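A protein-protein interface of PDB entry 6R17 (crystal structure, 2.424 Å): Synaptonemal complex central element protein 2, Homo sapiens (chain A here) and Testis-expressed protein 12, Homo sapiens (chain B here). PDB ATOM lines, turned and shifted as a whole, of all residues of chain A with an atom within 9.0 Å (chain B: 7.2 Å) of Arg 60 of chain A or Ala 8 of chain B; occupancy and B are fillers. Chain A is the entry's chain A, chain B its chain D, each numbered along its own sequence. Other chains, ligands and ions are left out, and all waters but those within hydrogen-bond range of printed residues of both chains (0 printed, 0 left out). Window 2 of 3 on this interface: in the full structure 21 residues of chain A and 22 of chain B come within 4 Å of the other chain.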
ATOM      1  N   LEU A  53       4.551 -11.306   9.756  1.00  0.00           N
ATOM      2  CA  LEU A  53       3.307 -11.282   8.990  1.00  0.00           C
ATOM      3  C   LEU A  53       2.884  -9.852   8.667  1.00  0.00           C
ATOM      4  O   LEU A  53       2.471  -9.556   7.536  1.00  0.00           O
ATOM      5  CB  LEU A  53       2.201 -12.007   9.755  1.00  0.00           C
ATOM      6  CG  LEU A  53       2.456 -13.475  10.099  1.00  0.00           C
ATOM      7  CD1 LEU A  53       1.333 -14.031  10.961  1.00  0.00           C
ATOM      8  CD2 LEU A  53       2.629 -14.302   8.836  1.00  0.00           C
ATOM      9  N   THR A  54       2.982  -8.954   9.652  1.00  0.00           N
ATOM     10  CA  THR A  54       2.706  -7.543   9.401  1.00  0.00           C
ATOM     11  C   THR A  54       3.650  -6.988   8.340  1.00  0.00           C
ATOM     12  O   THR A  54       3.245  -6.183   7.491  1.00  0.00           O
ATOM     13  CB  THR A  54       2.841  -6.745  10.698  1.00  0.00           C
ATOM     14  OG1 THR A  54       1.992  -7.314  11.701  1.00  0.00           O
ATOM     15  CG2 THR A  54       2.422  -5.299  10.476  1.00  0.00           C
ATOM     16  N   GLU A  55       4.911  -7.421   8.374  1.00  0.00           N
ATOM     17  CA  GLU A  55       5.899  -6.982   7.396  1.00  0.00           C
ATOM     18  C   GLU A  55       5.486  -7.377   5.983  1.00  0.00           C
ATOM     19  O   GLU A  55       5.535  -6.559   5.056  1.00  0.00           O
ATOM     20  CB  GLU A  55       7.260  -7.581   7.759  1.00  0.00           C
ATOM     21  CG  GLU A  55       8.425  -7.150   6.894  1.00  0.00           C
ATOM     22  CD  GLU A  55       9.698  -7.897   7.249  1.00  0.00           C
ATOM     23  OE1 GLU A  55       9.810  -8.367   8.402  1.00  0.00           O
ATOM     24  OE2 GLU A  55      10.585  -8.018   6.377  1.00  0.00           O
ATOM     25  N   LYS A  56       5.067  -8.631   5.802  1.00  0.00           N
ATOM     26  CA  LYS A  56       4.655  -9.079   4.471  1.00  0.00           C
ATOM     27  C   LYS A  56       3.378  -8.380   4.013  1.00  0.00           C
ATOM     28  O   LYS A  56       3.225  -8.068   2.822  1.00  0.00           O
ATOM     29  CB  LYS A  56       4.496 -10.599   4.445  1.00  0.00           C
ATOM     30  CG  LYS A  56       5.733 -11.325   4.943  1.00  0.00           C
ATOM     31  CD  LYS A  56       6.918 -11.013   4.040  1.00  0.00           C
ATOM     32  CE  LYS A  56       8.236 -11.103   4.791  1.00  0.00           C
ATOM     33  NZ  LYS A  56       9.338 -10.422   4.051  1.00  0.00           N
ATOM     34  N   LEU A  57       2.445  -8.131   4.938  1.00  0.00           N
ATOM     35  CA  LEU A  57       1.248  -7.374   4.579  1.00  0.00           C
ATOM     36  C   LEU A  57       1.616  -5.982   4.078  1.00  0.00           C
ATOM     37  O   LEU A  57       1.103  -5.522   3.047  1.00  0.00           O
ATOM     38  CB  LEU A  57       0.296  -7.280   5.771  1.00  0.00           C
ATOM     39  CG  LEU A  57      -0.707  -8.419   5.944  1.00  0.00           C
ATOM     40  CD1 LEU A  57      -1.654  -8.118   7.095  1.00  0.00           C
ATOM     41  CD2 LEU A  57      -1.482  -8.638   4.651  1.00  0.00           C
ATOM     42  N   GLU A  58       2.505  -5.296   4.802  1.00  0.00           N
ATOM     43  CA  GLU A  58       2.937  -3.973   4.367  1.00  0.00           C
ATOM     44  C   GLU A  58       3.652  -4.042   3.026  1.00  0.00           C
ATOM     45  O   GLU A  58       3.501  -3.145   2.192  1.00  0.00           O
ATOM     46  CB  GLU A  58       3.843  -3.335   5.420  1.00  0.00           C
ATOM     47  CG  GLU A  58       3.177  -3.110   6.764  1.00  0.00           C
ATOM     48  CD  GLU A  58       4.154  -2.652   7.827  1.00  0.00           C
ATOM     49  OE1 GLU A  58       3.698  -2.131   8.866  1.00  0.00           O
ATOM     50  OE2 GLU A  58       5.378  -2.799   7.620  1.00  0.00           O
ATOM     51  N   GLU A  59       4.415  -5.112   2.790  1.00  0.00           N
ATOM     52  CA  GLU A  59       5.100  -5.266   1.509  1.00  0.00           C
ATOM     53  C   GLU A  59       4.105  -5.361   0.353  1.00  0.00           C
ATOM     54  O   GLU A  59       4.240  -4.661  -0.661  1.00  0.00           O
ATOM     55  CB  GLU A  59       6.007  -6.498   1.561  1.00  0.00           C
ATOM     56  CG  GLU A  59       6.472  -7.015   0.212  1.00  0.00           C
ATOM     57  CD  GLU A  59       7.304  -8.279   0.340  1.00  0.00           C
ATOM     58  OE1 GLU A  59       7.563  -8.707   1.486  1.00  0.00           O
ATOM     59  OE2 GLU A  59       7.702  -8.841  -0.702  1.00  0.00           O
ATOM     60  N   ARG A  60       3.090  -6.220   0.492  1.00  0.00           N
ATOM     61  CA  ARG A  60       2.111  -6.359  -0.588  1.00  0.00           C
ATOM     62  C   ARG A  60       1.299  -5.083  -0.795  1.00  0.00           C
ATOM     63  O   ARG A  60       1.043  -4.678  -1.940  1.00  0.00           O
ATOM     64  CB  ARG A  60       1.178  -7.538  -0.326  1.00  0.00           C
ATOM     65  CG  ARG A  60       0.420  -7.952  -1.575  1.00  0.00           C
ATOM     66  CD  ARG A  60      -0.203  -9.329  -1.464  1.00  0.00           C
ATOM     67  NE  ARG A  60       0.757 -10.392  -1.756  1.00  0.00           N
ATOM     68  CZ  ARG A  60       1.241 -10.656  -2.968  1.00  0.00           C
ATOM     69  NH1 ARG A  60       0.871  -9.927  -4.013  1.00  0.00           N
ATOM     70  NH2 ARG A  60       2.105 -11.647  -3.133  1.00  0.00           N
ATOM     71  N   ILE A  61       0.882  -4.434   0.296  1.00  0.00           N
ATOM     72  CA  ILE A  61       0.134  -3.188   0.160  1.00  0.00           C
ATOM     73  C   ILE A  61       0.994  -2.128  -0.511  1.00  0.00           C
ATOM     74  O   ILE A  61       0.509  -1.335  -1.332  1.00  0.00           O
ATOM     75  CB  ILE A  61      -0.387  -2.730   1.531  1.00  0.00           C
ATOM     76  CG1 ILE A  61      -1.389  -3.755   2.060  1.00  0.00           C
ATOM     77  CG2 ILE A  61      -1.047  -1.369   1.415  1.00  0.00           C
ATOM     78  CD1 ILE A  61      -1.568  -3.725   3.549  1.00  0.00           C
ATOM     79  N   TYR A  62       2.284  -2.093  -0.173  1.00  0.00           N
ATOM     80  CA  TYR A  62       3.177  -1.142  -0.815  1.00  0.00           C
ATOM     81  C   TYR A  62       3.291  -1.420  -2.306  1.00  0.00           C
ATOM     82  O   TYR A  62       3.348  -0.486  -3.111  1.00  0.00           O
ATOM     83  CB  TYR A  62       4.560  -1.170  -0.169  1.00  0.00           C
ATOM     84  CG  TYR A  62       5.501  -0.258  -0.903  1.00  0.00           C
ATOM     85  CD1 TYR A  62       5.531   1.095  -0.611  1.00  0.00           C
ATOM     86  CD2 TYR A  62       6.332  -0.735  -1.911  1.00  0.00           C
ATOM     87  CE1 TYR A  62       6.361   1.946  -1.287  1.00  0.00           C
ATOM     88  CE2 TYR A  62       7.171   0.114  -2.595  1.00  0.00           C
ATOM     89  CZ  TYR A  62       7.178   1.453  -2.272  1.00  0.00           C
ATOM     90  OH  TYR A  62       7.998   2.320  -2.933  1.00  0.00           O
ATOM     91  N   GLN A  63       3.358  -2.696  -2.693  1.00  0.00           N
ATOM     92  CA  GLN A  63       3.408  -3.013  -4.119  1.00  0.00           C
ATOM     93  C   GLN A  63       2.144  -2.543  -4.832  1.00  0.00           C
ATOM     94  O   GLN A  63       2.208  -2.015  -5.952  1.00  0.00           O
ATOM     95  CB  GLN A  63       3.626  -4.513  -4.324  1.00  0.00           C
ATOM     96  CG  GLN A  63       5.058  -4.973  -4.083  1.00  0.00           C
ATOM     97  CD  GLN A  63       6.057  -4.276  -4.991  1.00  0.00           C
ATOM     98  OE1 GLN A  63       6.566  -3.202  -4.667  1.00  0.00           O
ATOM     99  NE2 GLN A  63       6.345  -4.888  -6.135  1.00  0.00           N
ATOM    100  N   ILE A  64       0.985  -2.711  -4.189  1.00  0.00           N
ATOM    101  CA  ILE A  64      -0.267  -2.238  -4.781  1.00  0.00           C
ATOM    102  C   ILE A  64      -0.234  -0.723  -4.966  1.00  0.00           C
ATOM    103  O   ILE A  64      -0.598  -0.199  -6.029  1.00  0.00           O
ATOM    104  CB  ILE A  64      -1.469  -2.677  -3.926  1.00  0.00           C
ATOM    105  CG1 ILE A  64      -1.540  -4.203  -3.852  1.00  0.00           C
ATOM    106  CG2 ILE A  64      -2.763  -2.099  -4.484  1.00  0.00           C
ATOM    107  CD1 ILE A  64      -2.686  -4.716  -3.013  1.00  0.00           C
ATOM    108  N   TYR A  65       0.210   0.004  -3.936  1.00  0.00           N
ATOM    109  CA  TYR A  65       0.280   1.461  -4.037  1.00  0.00           C
ATOM    110  C   TYR A  65       1.293   1.908  -5.086  1.00  0.00           C
ATOM    111  O   TYR A  65       1.080   2.909  -5.779  1.00  0.00           O
ATOM    112  CB  TYR A  65       0.633   2.079  -2.684  1.00  0.00           C
ATOM    113  CG  TYR A  65      -0.547   2.469  -1.824  1.00  0.00           C
ATOM    114  CD1 TYR A  65      -0.352   2.959  -0.540  1.00  0.00           C
ATOM    115  CD2 TYR A  65      -1.849   2.368  -2.296  1.00  0.00           C
ATOM    116  CE1 TYR A  65      -1.418   3.329   0.255  1.00  0.00           C
ATOM    117  CE2 TYR A  65      -2.925   2.737  -1.503  1.00  0.00           C
ATOM    118  CZ  TYR A  65      -2.700   3.215  -0.228  1.00  0.00           C
ATOM    119  OH  TYR A  65      -3.755   3.587   0.574  1.00  0.00           O
ATOM    120  N   ASN A  66       2.409   1.188  -5.207  1.00  0.00           N
ATOM    121  CA  ASN A  66       3.408   1.532  -6.214  1.00  0.00           C
ATOM    122  C   ASN A  66       2.852   1.355  -7.619  1.00  0.00           C
ATOM    123  O   ASN A  66       3.076   2.198  -8.496  1.00  0.00           O
ATOM    124  CB  ASN A  66       4.665   0.683  -6.013  1.00  0.00           C
ATOM    125  CG  ASN A  66       5.580   0.691  -7.225  1.00  0.00           C
ATOM    126  OD1 ASN A  66       5.797   1.730  -7.852  1.00  0.00           O
ATOM    127  ND2 ASN A  66       6.127  -0.472  -7.557  1.00  0.00           N
ATOM    128  N   ASP A  67       2.122   0.261  -7.854  1.00  0.00           N
ATOM    129  CA  ASP A  67       1.487   0.077  -9.156  1.00  0.00           C
ATOM    130  C   ASP A  67       0.444   1.159  -9.419  1.00  0.00           C
ATOM    131  O   ASP A  67       0.321   1.656 -10.548  1.00  0.00           O
ATOM    132  CB  ASP A  67       0.864  -1.316  -9.239  1.00  0.00           C
ATOM    133  CG  ASP A  67       1.908  -2.415  -9.289  1.00  0.00           C
ATOM    134  OD1 ASP A  67       3.102  -2.109  -9.078  1.00  0.00           O
ATOM    135  OD2 ASP A  67       1.540  -3.582  -9.538  1.00  0.00           O
ATOM    136  N   ASP B   6      -4.957  -7.147  -5.745  1.00  0.00           N
ATOM    137  CA  ASP B   6      -6.143  -7.078  -4.900  1.00  0.00           C
ATOM    138  C   ASP B   6      -6.534  -8.467  -4.409  1.00  0.00           C
ATOM    139  O   ASP B   6      -6.878  -8.651  -3.241  1.00  0.00           O
ATOM    140  CB  ASP B   6      -7.309  -6.447  -5.666  1.00  0.00           C
ATOM    141  CG  ASP B   6      -7.103  -4.968  -5.929  1.00  0.00           C
ATOM    142  OD1 ASP B   6      -6.237  -4.358  -5.268  1.00  0.00           O
ATOM    143  OD2 ASP B   6      -7.799  -4.419  -6.809  1.00  0.00           O
ATOM    144  N   GLU B   7      -6.486  -9.441  -5.320  1.00  0.00           N
ATOM    145  CA  GLU B   7      -6.794 -10.822  -4.961  1.00  0.00           C
ATOM    146  C   GLU B   7      -5.796 -11.336  -3.930  1.00  0.00           C
ATOM    147  O   GLU B   7      -6.174 -11.932  -2.909  1.00  0.00           O
ATOM    148  CB  GLU B   7      -6.769 -11.693  -6.222  1.00  0.00           C
ATOM    149  CG  GLU B   7      -7.267 -13.125  -6.055  1.00  0.00           C
ATOM    150  CD  GLU B   7      -6.337 -14.063  -5.310  1.00  0.00           C
ATOM    151  OE1 GLU B   7      -5.107 -13.856  -5.334  1.00  0.00           O
ATOM    152  OE2 GLU B   7      -6.858 -15.009  -4.679  1.00  0.00           O
ATOM    153  N   ALA B   8      -4.507 -11.108  -4.192  1.00  0.00           N
ATOM    154  CA  ALA B   8      -3.458 -11.531  -3.273  1.00  0.00           C
ATOM    155  C   ALA B   8      -3.606 -10.860  -1.915  1.00  0.00           C
ATOM    156  O   ALA B   8      -3.305 -11.467  -0.883  1.00  0.00           O
ATOM    157  CB  ALA B   8      -2.086 -11.239  -3.878  1.00  0.00           C
ATOM    158  N   LEU B   9      -4.042  -9.597  -1.896  1.00  0.00           N
ATOM    159  CA  LEU B   9      -4.270  -8.921  -0.622  1.00  0.00           C
ATOM    160  C   LEU B   9      -5.334  -9.642   0.197  1.00  0.00           C
ATOM    161  O   LEU B   9      -5.167  -9.837   1.407  1.00  0.00           O
ATOM    162  CB  LEU B   9      -4.669  -7.464  -0.857  1.00  0.00           C
ATOM    163  CG  LEU B   9      -4.980  -6.659   0.404  1.00  0.00           C
ATOM    164  CD1 LEU B   9      -3.738  -6.518   1.271  1.00  0.00           C
ATOM    165  CD2 LEU B   9      -5.545  -5.293   0.043  1.00  0.00           C
ATOM    166  N   GLU B  10      -6.421 -10.069  -0.451  1.00  0.00           N
ATOM    167  CA  GLU B  10      -7.465 -10.808   0.251  1.00  0.00           C
ATOM    168  C   GLU B  10      -6.921 -12.126   0.784  1.00  0.00           C
ATOM    169  O   GLU B  10      -7.098 -12.464   1.967  1.00  0.00           O
ATOM    170  CB  GLU B  10      -8.646 -11.064  -0.693  1.00  0.00           C
ATOM    171  CG  GLU B  10      -9.263  -9.822  -1.346  1.00  0.00           C
ATOM    172  CD  GLU B  10      -9.930  -8.867  -0.369  1.00  0.00           C
ATOM    173  OE1 GLU B  10     -10.021  -9.184   0.835  1.00  0.00           O
ATOM    174  OE2 GLU B  10     -10.363  -7.782  -0.812  1.00  0.00           O
ATOM    175  N   LYS B  11      -6.249 -12.886  -0.091  1.00  0.00           N
ATOM    176  CA  LYS B  11      -5.679 -14.169   0.311  1.00  0.00           C
ATOM    177  C   LYS B  11      -4.755 -14.009   1.511  1.00  0.00           C
ATOM    178  O   LYS B  11      -4.840 -14.773   2.480  1.00  0.00           O
ATOM    179  CB  LYS B  11      -4.922 -14.801  -0.859  1.00  0.00           C
ATOM    180  CG  LYS B  11      -4.416 -16.210  -0.575  1.00  0.00           C
ATOM    181  CD  LYS B  11      -3.449 -16.695  -1.648  1.00  0.00           C
ATOM    182  CE  LYS B  11      -2.029 -16.227  -1.372  1.00  0.00           C
ATOM    183  NZ  LYS B  11      -1.110 -17.379  -1.153  1.00  0.00           N
ATOM    184  N   ASP B  12      -3.878 -13.003   1.475  1.00  0.00           N
ATOM    185  CA  ASP B  12      -2.873 -12.867   2.519  1.00  0.00           C
ATOM    186  C   ASP B  12      -3.446 -12.302   3.807  1.00  0.00           C
ATOM    187  O   ASP B  12      -2.983 -12.665   4.889  1.00  0.00           O
ATOM    188  CB  ASP B  12      -1.726 -11.978   2.039  1.00  0.00           C
ATOM    189  CG  ASP B  12      -0.873 -12.650   0.992  1.00  0.00           C
ATOM    190  OD1 ASP B  12      -1.083 -13.855   0.741  1.00  0.00           O
ATOM    191  OD2 ASP B  12       0.012 -11.977   0.425  1.00  0.00           O
ATOM    192  N   LEU B  13      -4.462 -11.441   3.722  1.00  0.00           N
ATOM    193  CA  LEU B  13      -5.162 -10.999   4.921  1.00  0.00           C
ATOM    194  C   LEU B  13      -5.807 -12.175   5.645  1.00  0.00           C
ATOM    195  O   LEU B  13      -5.617 -12.366   6.858  1.00  0.00           O
ATOM    196  CB  LEU B  13      -6.219  -9.969   4.524  1.00  0.00           C
ATOM    197  CG  LEU B  13      -5.777  -8.504   4.477  1.00  0.00           C
ATOM    198  CD1 LEU B  13      -6.969  -7.596   4.242  1.00  0.00           C
ATOM    199  CD2 LEU B  13      -5.041  -8.099   5.743  1.00  0.00           C
ATOM    200  N   ASN B  14      -6.522 -13.018   4.890  1.00  0.00           N
ATOM    201  CA  ASN B  14      -7.164 -14.180   5.496  1.00  0.00           C
ATOM    202  C   ASN B  14      -6.132 -15.150   6.056  1.00  0.00           C
ATOM    203  O   ASN B  14      -6.303 -15.682   7.161  1.00  0.00           O
ATOM    204  CB  ASN B  14      -8.054 -14.874   4.464  1.00  0.00           C
ATOM    205  CG  ASN B  14      -9.402 -14.193   4.303  1.00  0.00           C
ATOM    206  OD1 ASN B  14      -9.888 -13.518   5.213  1.00  0.00           O
ATOM    207  ND2 ASN B  14     -10.004 -14.353   3.131  1.00  0.00           N
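Among the printed residues, pairs that only touch across the chains: Arg 60 of chain A with Ala 8 of chain B (3.2 Å), Leu 57 of chain A with Leu 13 of chain B (3.6 Å), Ile 61 of chain A with Leu 9 of chain B (3.7 Å) and Arg 60 of chain A with Leu 9 of chain B (3.9 Å).
NE of Arg 60 of chain A lies within salt-bridge range of OD2 of Asp 12 of chain B (2.8 Å).
Of chain B, only Ala 8 (3.2 Å), Leu 9 (3.9 Å) and Asp 12 (2.8 Å) come within 4 Å of Arg 60 of chain A.
Of chain A, only Arg 60 comes within 4 Å of Ala 8 of chain B.
Of the printed residues of chain A, Leu 13 of chain B touches Leu 57.
Printed residues of chain B within 4 Å of Leu 57 of chain A: Leu 13.
Of the printed residues of chain A, Leu 9 of chain B touches Arg 60 and Ile 61.
Ile 64 of chain A touches none of the printed residues of chain B.
Asp 6 of chain B touches none of the printed residues of chain A.
The nearest residue of chain B that does not touch Arg 60 of chain A is Glu 10 of chain B (6.3 Å).
Hydrophobic or aromatic side chains of chain A that line the printed part of chain B: Leu 57 and Ile 61.
Of the 9 printed residues of chain B, 4 touch a printed residue of chain A.
Along chain B the printed residues that touch a printed residue of chain A span positions 8 to 13.
Among the printed residues, Asp or Glu carboxylates within 4 Å of a Lys or Arg side-chain nitrogen of the other chain: Arg 60 of chain A with Asp 12 of chain B.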
